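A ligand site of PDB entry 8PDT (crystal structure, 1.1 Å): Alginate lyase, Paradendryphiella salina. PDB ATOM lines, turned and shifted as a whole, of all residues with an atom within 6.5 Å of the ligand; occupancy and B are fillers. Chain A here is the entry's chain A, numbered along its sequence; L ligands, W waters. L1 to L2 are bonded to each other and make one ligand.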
ATOM      1  N   SER A  60     -24.987  -6.585   0.278  1.00  0.00           N
ATOM      2  CA  SER A  60     -23.774  -5.814   0.499  1.00  0.00           C
ATOM      3  C   SER A  60     -22.844  -6.437   1.529  1.00  0.00           C
ATOM      4  O   SER A  60     -21.827  -5.838   1.861  1.00  0.00           O
ATOM      5  CB  SER A  60     -24.037  -4.340   0.844  1.00  0.00           C
ATOM      6  N   GLU A 103     -25.866 -11.214  -8.033  1.00  0.00           N
ATOM      7  CA  GLU A 103     -24.597 -10.666  -8.492  1.00  0.00           C
ATOM      8  C   GLU A 103     -23.583 -10.880  -7.388  1.00  0.00           C
ATOM      9  O   GLU A 103     -23.866 -10.612  -6.221  1.00  0.00           O
ATOM     10  CB  GLU A 103     -24.698  -9.178  -8.860  1.00  0.00           C
ATOM     11  CG  GLU A 103     -23.327  -8.622  -9.310  1.00  0.00           C
ATOM     12  CD  GLU A 103     -23.327  -7.200  -9.794  1.00  0.00           C
ATOM     13  OE1 GLU A 103     -24.342  -6.504  -9.641  1.00  0.00           O
ATOM     14  OE2 GLU A 103     -22.261  -6.748 -10.321  1.00  0.00           O
ATOM     15  N   THR A 105     -19.525 -10.090  -6.618  1.00  0.00           N
ATOM     16  CA  THR A 105     -18.230  -9.538  -6.986  1.00  0.00           C
ATOM     17  C   THR A 105     -17.129 -10.463  -6.468  1.00  0.00           C
ATOM     18  O   THR A 105     -17.083 -10.772  -5.278  1.00  0.00           O
ATOM     19  CB  THR A 105     -18.111  -8.122  -6.395  1.00  0.00           C
ATOM     20  OG1 THR A 105     -19.067  -7.260  -6.996  1.00  0.00           O
ATOM     21  CG2 THR A 105     -16.730  -7.531  -6.635  1.00  0.00           C
ATOM     22  N   GLN A 108     -11.765  -7.131  -7.174  1.00  0.00           N
ATOM     23  CA  GLN A 108     -11.921  -5.680  -7.266  1.00  0.00           C
ATOM     24  C   GLN A 108     -10.566  -4.986  -7.336  1.00  0.00           C
ATOM     25  O   GLN A 108      -9.554  -5.476  -6.845  1.00  0.00           O
ATOM     26  CB  GLN A 108     -12.623  -5.088  -6.034  1.00  0.00           C
ATOM     27  CG  GLN A 108     -13.981  -5.686  -5.725  1.00  0.00           C
ATOM     28  CD  GLN A 108     -14.812  -4.789  -4.813  1.00  0.00           C
ATOM     29  OE1 GLN A 108     -15.096  -3.633  -5.149  1.00  0.00           O
ATOM     30  NE2 GLN A 108     -15.188  -5.309  -3.660  1.00  0.00           N
ATOM     31  N   HIS A 110     -10.240  -1.363  -5.581  1.00  0.00           N
ATOM     32  CA  HIS A 110     -11.025  -0.455  -4.759  1.00  0.00           C
ATOM     33  C   HIS A 110     -10.099   0.557  -4.111  1.00  0.00           C
ATOM     34  O   HIS A 110      -8.904   0.313  -3.922  1.00  0.00           O
ATOM     35  CB  HIS A 110     -11.791  -1.244  -3.665  1.00  0.00           C
ATOM     36  CG  HIS A 110     -13.065  -0.610  -3.212  1.00  0.00           C
ATOM     37  ND1 HIS A 110     -13.088   0.492  -2.370  1.00  0.00           N
ATOM     38  CD2 HIS A 110     -14.348  -0.925  -3.456  1.00  0.00           C
ATOM     39  CE1 HIS A 110     -14.348   0.821  -2.141  1.00  0.00           C
ATOM     40  NE2 HIS A 110     -15.141  -0.011  -2.792  1.00  0.00           N
ATOM     41  N   PRO A 115     -15.168   1.748  -5.918  1.00  0.00           N
ATOM     42  CA  PRO A 115     -14.628   0.644  -6.706  1.00  0.00           C
ATOM     43  C   PRO A 115     -14.193   1.112  -8.091  1.00  0.00           C
ATOM     44  O   PRO A 115     -15.026   1.455  -8.946  1.00  0.00           O
ATOM     45  CB  PRO A 115     -15.830  -0.314  -6.809  1.00  0.00           C
ATOM     46  CG  PRO A 115     -17.033   0.615  -6.825  1.00  0.00           C
ATOM     47  CD  PRO A 115     -16.644   1.786  -5.948  1.00  0.00           C
ATOM     48  N   ARG A 118     -14.926  -3.730 -10.573  1.00  0.00           N
ATOM     49  CA  ARG A 118     -15.483  -4.969 -10.052  1.00  0.00           C
ATOM     50  C   ARG A 118     -15.570  -5.985 -11.187  1.00  0.00           C
ATOM     51  O   ARG A 118     -16.145  -5.689 -12.238  1.00  0.00           O
ATOM     52  CB  ARG A 118     -16.886  -4.772  -9.468  1.00  0.00           C
ATOM     53  CG  ARG A 118     -16.935  -3.785  -8.290  1.00  0.00           C
ATOM     54  CD  ARG A 118     -18.324  -3.685  -7.659  1.00  0.00           C
ATOM     55  NE  ARG A 118     -19.356  -3.338  -8.624  1.00  0.00           N
ATOM     56  CZ  ARG A 118     -20.209  -4.202  -9.168  1.00  0.00           C
ATOM     57  NH1 ARG A 118     -20.206  -5.478  -8.840  1.00  0.00           N
ATOM     58  NH2 ARG A 118     -21.063  -3.781 -10.081  1.00  0.00           N
ATOM     59  N   LYS A 125     -28.374  -9.576 -17.086  1.00  0.00           N
ATOM     60  CA  LYS A 125     -28.150  -8.152 -17.298  1.00  0.00           C
ATOM     61  C   LYS A 125     -28.068  -7.861 -18.784  1.00  0.00           C
ATOM     62  O   LYS A 125     -27.546  -8.685 -19.546  1.00  0.00           O
ATOM     63  CB  LYS A 125     -26.859  -7.715 -16.605  1.00  0.00           C
ATOM     64  CG  LYS A 125     -26.535  -6.221 -16.674  1.00  0.00           C
ATOM     65  CD  LYS A 125     -27.540  -5.380 -15.905  1.00  0.00           C
ATOM     66  CE  LYS A 125     -27.096  -3.915 -15.876  1.00  0.00           C
ATOM     67  NZ  LYS A 125     -28.118  -2.989 -15.289  1.00  0.00           N
ATOM     68  N   MET A 137     -18.806 -10.294 -15.630  1.00  0.00           N
ATOM     69  CA  MET A 137     -18.859  -8.915 -16.098  1.00  0.00           C
ATOM     70  C   MET A 137     -17.736  -8.111 -15.465  1.00  0.00           C
ATOM     71  O   MET A 137     -17.337  -8.357 -14.319  1.00  0.00           O
ATOM     72  CB  MET A 137     -20.199  -8.285 -15.633  1.00  0.00           C
ATOM     73  CG  MET A 137     -20.435  -6.837 -16.029  1.00  0.00           C
ATOM     74  SD  MET A 137     -22.163  -6.407 -15.685  1.00  0.00           S
ATOM     75  CE  MET A 137     -22.187  -6.487 -13.912  1.00  0.00           C
ATOM     76  N   THR A 139     -17.100  -4.121 -14.413  1.00  0.00           N
ATOM     77  CA  THR A 139     -17.683  -2.794 -14.222  1.00  0.00           C
ATOM     78  C   THR A 139     -16.551  -1.873 -13.795  1.00  0.00           C
ATOM     79  O   THR A 139     -16.000  -2.010 -12.699  1.00  0.00           O
ATOM     80  CB  THR A 139     -18.786  -2.815 -13.176  1.00  0.00           C
ATOM     81  OG1 THR A 139     -19.848  -3.691 -13.603  1.00  0.00           O
ATOM     82  CG2 THR A 139     -19.352  -1.426 -12.990  1.00  0.00           C
ATOM     83  N   ARG A 141     -15.427   2.062 -13.081  1.00  0.00           N
ATOM     84  CA  ARG A 141     -15.855   3.441 -12.866  1.00  0.00           C
ATOM     85  C   ARG A 141     -14.883   4.405 -13.526  1.00  0.00           C
ATOM     86  O   ARG A 141     -13.671   4.324 -13.291  1.00  0.00           O
ATOM     87  CB  ARG A 141     -16.003   3.787 -11.390  1.00  0.00           C
ATOM     88  CG  ARG A 141     -17.340   3.417 -10.816  1.00  0.00           C
ATOM     89  CD  ARG A 141     -17.500   3.921  -9.376  1.00  0.00           C
ATOM     90  NE  ARG A 141     -18.861   3.789  -8.852  1.00  0.00           N
ATOM     91  CZ  ARG A 141     -19.825   4.681  -9.039  1.00  0.00           C
ATOM     92  NH1 ARG A 141     -19.615   5.782  -9.732  1.00  0.00           N
ATOM     93  NH2 ARG A 141     -21.027   4.460  -8.500  1.00  0.00           N
ATOM     94  N   ASP A 146     -23.719   8.614 -10.685  1.00  0.00           N
ATOM     95  CA  ASP A 146     -24.584   7.440 -10.742  1.00  0.00           C
ATOM     96  C   ASP A 146     -25.075   7.122 -12.141  1.00  0.00           C
ATOM     97  O   ASP A 146     -25.538   5.992 -12.374  1.00  0.00           O
ATOM     98  CB  ASP A 146     -25.808   7.628  -9.836  1.00  0.00           C
ATOM     99  CG  ASP A 146     -26.677   8.811 -10.246  1.00  0.00           C
ATOM    100  OD1 ASP A 146     -26.252   9.978 -10.035  1.00  0.00           O
ATOM    101  OD2 ASP A 146     -27.778   8.582 -10.781  1.00  0.00           O
ATOM    102  N   PHE A 151     -19.645   4.690 -15.980  1.00  0.00           N
ATOM    103  CA  PHE A 151     -19.250   3.283 -15.965  1.00  0.00           C
ATOM    104  C   PHE A 151     -18.933   2.821 -17.381  1.00  0.00           C
ATOM    105  O   PHE A 151     -19.544   3.277 -18.350  1.00  0.00           O
ATOM    106  CB  PHE A 151     -20.403   2.403 -15.461  1.00  0.00           C
ATOM    107  CG  PHE A 151     -20.916   2.781 -14.101  1.00  0.00           C
ATOM    108  CD1 PHE A 151     -20.361   2.245 -12.951  1.00  0.00           C
ATOM    109  CD2 PHE A 151     -21.963   3.695 -13.969  1.00  0.00           C
ATOM    110  CE1 PHE A 151     -20.833   2.603 -11.694  1.00  0.00           C
ATOM    111  CE2 PHE A 151     -22.453   4.041 -12.717  1.00  0.00           C
ATOM    112  CZ  PHE A 151     -21.892   3.495 -11.586  1.00  0.00           C
ATOM    113  N   LYS A 153     -19.076  -1.002 -18.740  1.00  0.00           N
ATOM    114  CA  LYS A 153     -19.466  -2.353 -18.368  1.00  0.00           C
ATOM    115  C   LYS A 153     -19.270  -3.281 -19.567  1.00  0.00           C
ATOM    116  O   LYS A 153     -19.716  -2.967 -20.675  1.00  0.00           O
ATOM    117  CB  LYS A 153     -20.902  -2.390 -17.866  1.00  0.00           C
ATOM    118  CG  LYS A 153     -21.082  -1.590 -16.578  1.00  0.00           C
ATOM    119  CD  LYS A 153     -22.535  -1.391 -16.186  1.00  0.00           C
ATOM    120  CE  LYS A 153     -23.129  -2.620 -15.540  1.00  0.00           C
ATOM    121  NZ  LYS A 153     -22.707  -2.747 -14.107  1.00  0.00           N
ATOM    122  N   TYR A 206     -18.447 -10.815  -2.663  1.00  0.00           N
ATOM    123  CA  TYR A 206     -19.121  -9.617  -2.195  1.00  0.00           C
ATOM    124  C   TYR A 206     -20.493  -9.597  -2.871  1.00  0.00           C
ATOM    125  O   TYR A 206     -20.568  -9.552  -4.110  1.00  0.00           O
ATOM    126  CB  TYR A 206     -18.240  -8.400  -2.498  1.00  0.00           C
ATOM    127  CG  TYR A 206     -18.853  -7.045  -2.357  1.00  0.00           C
ATOM    128  CD1 TYR A 206     -19.722  -6.720  -1.307  1.00  0.00           C
ATOM    129  CD2 TYR A 206     -18.519  -6.051  -3.274  1.00  0.00           C
ATOM    130  CE1 TYR A 206     -20.239  -5.429  -1.191  1.00  0.00           C
ATOM    131  CE2 TYR A 206     -19.042  -4.772  -3.169  1.00  0.00           C
ATOM    132  CZ  TYR A 206     -19.885  -4.464  -2.133  1.00  0.00           C
ATOM    133  OH  TYR A 206     -20.385  -3.173  -2.042  1.00  0.00           O
ATOM    134  N   ASN A 208     -24.063  -8.590  -4.111  1.00  0.00           N
ATOM    135  CA  ASN A 208     -24.680  -7.370  -4.574  1.00  0.00           C
ATOM    136  C   ASN A 208     -26.127  -7.601  -5.031  1.00  0.00           C
ATOM    137  O   ASN A 208     -26.409  -8.512  -5.806  1.00  0.00           O
ATOM    138  CB  ASN A 208     -23.897  -6.782  -5.745  1.00  0.00           C
ATOM    139  CG  ASN A 208     -22.384  -6.844  -5.549  1.00  0.00           C
ATOM    140  OD1 ASN A 208     -21.676  -7.456  -6.362  1.00  0.00           O
ATOM    141  ND2 ASN A 208     -21.887  -6.252  -4.461  1.00  0.00           N
ATOM    142  N   ASN A 209     -27.034  -6.761  -4.567  1.00  0.00           N
ATOM    143  CA  ASN A 209     -28.431  -6.777  -5.000  1.00  0.00           C
ATOM    144  C   ASN A 209     -29.124  -8.148  -4.986  1.00  0.00           C
ATOM    145  O   ASN A 209     -29.813  -8.499  -5.943  1.00  0.00           O
ATOM    146  CB  ASN A 209     -28.592  -6.159  -6.381  1.00  0.00           C
ATOM    147  CG  ASN A 209     -28.106  -4.734  -6.454  1.00  0.00           C
ATOM    148  OD1 ASN A 209     -28.249  -3.949  -5.510  1.00  0.00           O
ATOM    149  ND2 ASN A 209     -27.541  -4.371  -7.605  1.00  0.00           N
HETATM  150  C1  LIG L   1     -21.149  -1.495  -4.724  1.00  0.00           C
HETATM  151  O1  LIG L   1     -20.154  -2.189  -5.174  1.00  0.00           O
HETATM  152  C2  LIG L   1     -22.466  -2.178  -5.153  1.00  0.00           C
HETATM  153  O2  LIG L   1     -23.560  -1.439  -4.628  1.00  0.00           O
HETATM  154  C3  LIG L   1     -22.588  -2.251  -6.634  1.00  0.00           C
HETATM  155  O3  LIG L   1     -23.888  -2.880  -6.954  1.00  0.00           O
HETATM  156  C4  LIG L   1     -22.464  -0.924  -7.270  1.00  0.00           C
HETATM  157  O4  LIG L   1     -22.357  -1.161  -8.705  1.00  0.00           O
HETATM  158  C5  LIG L   1     -21.201  -0.245  -6.836  1.00  0.00           C
HETATM  159  O5  LIG L   1     -21.151  -0.107  -5.375  1.00  0.00           O
HETATM  160  C6  LIG L   1     -21.078   1.144  -7.409  1.00  0.00           C
HETATM  161  O6  LIG L   1     -20.247   1.360  -8.326  1.00  0.00           O
HETATM  162  O7  LIG L   1     -21.799   2.058  -6.923  1.00  0.00           O
HETATM  163  C1  LG2 L   2     -23.241  -0.409  -9.493  1.00  0.00           C
HETATM  164  C2  LG2 L   2     -22.873  -0.528 -10.958  1.00  0.00           C
HETATM  165  O1  LG2 L   2     -22.812  -1.926 -11.310  1.00  0.00           O
HETATM  166  C3  LG2 L   2     -23.882   0.133 -11.834  1.00  0.00           C
HETATM  167  O2  LG2 L   2     -23.526  -0.175 -13.208  1.00  0.00           O
HETATM  168  C4  LG2 L   2     -25.279  -0.317 -11.537  1.00  0.00           C
HETATM  169  O3  LG2 L   2     -26.206   0.545 -12.203  1.00  0.00           O
HETATM  170  C5  LG2 L   2     -25.608  -0.314 -10.029  1.00  0.00           C
HETATM  171  O4  LG2 L   2     -24.582  -0.935  -9.190  1.00  0.00           O
HETATM  172  C6  LG2 L   2     -26.840  -1.115  -9.777  1.00  0.00           C
HETATM  173  O5  LG2 L   2     -27.921  -0.504  -9.591  1.00  0.00           O
HETATM  174  O6  LG2 L   2     -26.791  -2.374  -9.727  1.00  0.00           O
HETATM  175  O   HOH W   1     -28.205  -4.540 -11.094  1.00  0.00           O
HETATM  176  O   HOH W   2     -23.239  -1.469  -1.746  1.00  0.00           O
HETATM  177  O   HOH W   3     -24.633  -4.448 -12.584  1.00  0.00           O
HETATM  178  O   HOH W   4     -19.214  -0.758  -9.727  1.00  0.00           O
HETATM  179  O   HOH W   5     -24.308  -3.776  -9.683  1.00  0.00           O
HETATM  180  O   HOH W   6     -27.352   0.189  -6.964  1.00  0.00           O
HETATM  181  O   HOH W   7     -24.637   1.506 -15.157  1.00  0.00           O
HETATM  182  O   HOH W   8     -24.057   3.097  -8.087  1.00  0.00           O
HETATM  183  O   HOH W   9     -22.094   1.023  -2.321  1.00  0.00           O
HETATM  184  O   HOH W  10     -26.358  -1.800  -5.359  1.00  0.00           O
HETATM  185  O   HOH W  11     -18.120  -0.961  -3.282  1.00  0.00           O
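CG of Pro 115 touches O6 of LIG L1 (3.6 Å).
CG2 of Thr 139 touches O1 of LG2 L2, 3.9 Å away.
Phe 151 touches the ligand.
Hydrophobic or aromatic side chains that line the ligand: Pro 115, Phe 151 and Tyr 206.
Of the 17 residues printed, 8 come within 4 Å of the ligand.
The side-chain amide nitrogen (ND2) of Asn 209 lies within hydrogen-bond range of an oxygen (O6) of LG2 L2.
NE of Arg 141 lies within salt-bridge range of O6 of LIG L1 (2.8 Å).
An oxygen (O1) of LIG L1 lies close to the side-chain hydroxyl of Tyr 206 (3.3 Å).
An oxygen (O2) of LG2 L2 lies within hydrogen-bond range of the side-chain amino group of Lys 153.
O1 of LG2 L2 sits at hydrogen-bond distance from NH2 of Arg 118 (2.8 Å).
The guanidinium group (NH1) of Arg 118 is in salt-bridge range of the side-chain carboxylate (OE2) of Glu 103 (2.8 Å).
The backbone carbonyl oxygen (O) of Tyr 206 sits close to the side-chain amide oxygen (OD1) of Asn 208.
The side-chain amide oxygen (OD1) of Asn 208 sits at hydrogen-bond distance from the guanidinium group (NH1) of Arg 118 (3.5 Å).
NH1 of Arg 118 sits at hydrogen-bond distance from OG1 of Thr 105 (2.8 Å).
The side-chain amino group of Lys 153 lies within hydrogen-bond range of the side-chain hydroxyl of Thr 139, at 3.1 Å.
The backbone NH (N) of Thr 105 lies within hydrogen-bond range of the backbone carbonyl oxygen (O) of Tyr 206 (2.8 Å).
O of Arg 118 is in hydrogen-bond range of N of Thr 139, at 2.8 Å.
Water W4 bridges an oxygen (O6) of LIG L1 (2.7 Å) and the guanidinium group of Arg 118 (2.8 Å).
Water W5 lies within hydrogen-bond range of OE1 of Glu 103 (2.7 Å), O6 of LG2 L2 (2.9 Å) and NH2 of Arg 118 (3.3 Å).
Water W2 lies within hydrogen-bond range of O2 of LIG L1 (2.9 Å) and OH of Tyr 206 (3.3 Å).
Water W10 bridges the side-chain amide oxygen of Asn 209 (2.9 Å) and an oxygen (O2) of LIG L1 (2.9 Å).
Water W11 lies within hydrogen-bond range of an oxygen (O1) of LIG L1, a ring nitrogen (NE2) of His 110 and the side-chain hydroxyl (OH) of Tyr 206.
Water W3 bridges NZ of Lys 153 and O1 of LG2 L2.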
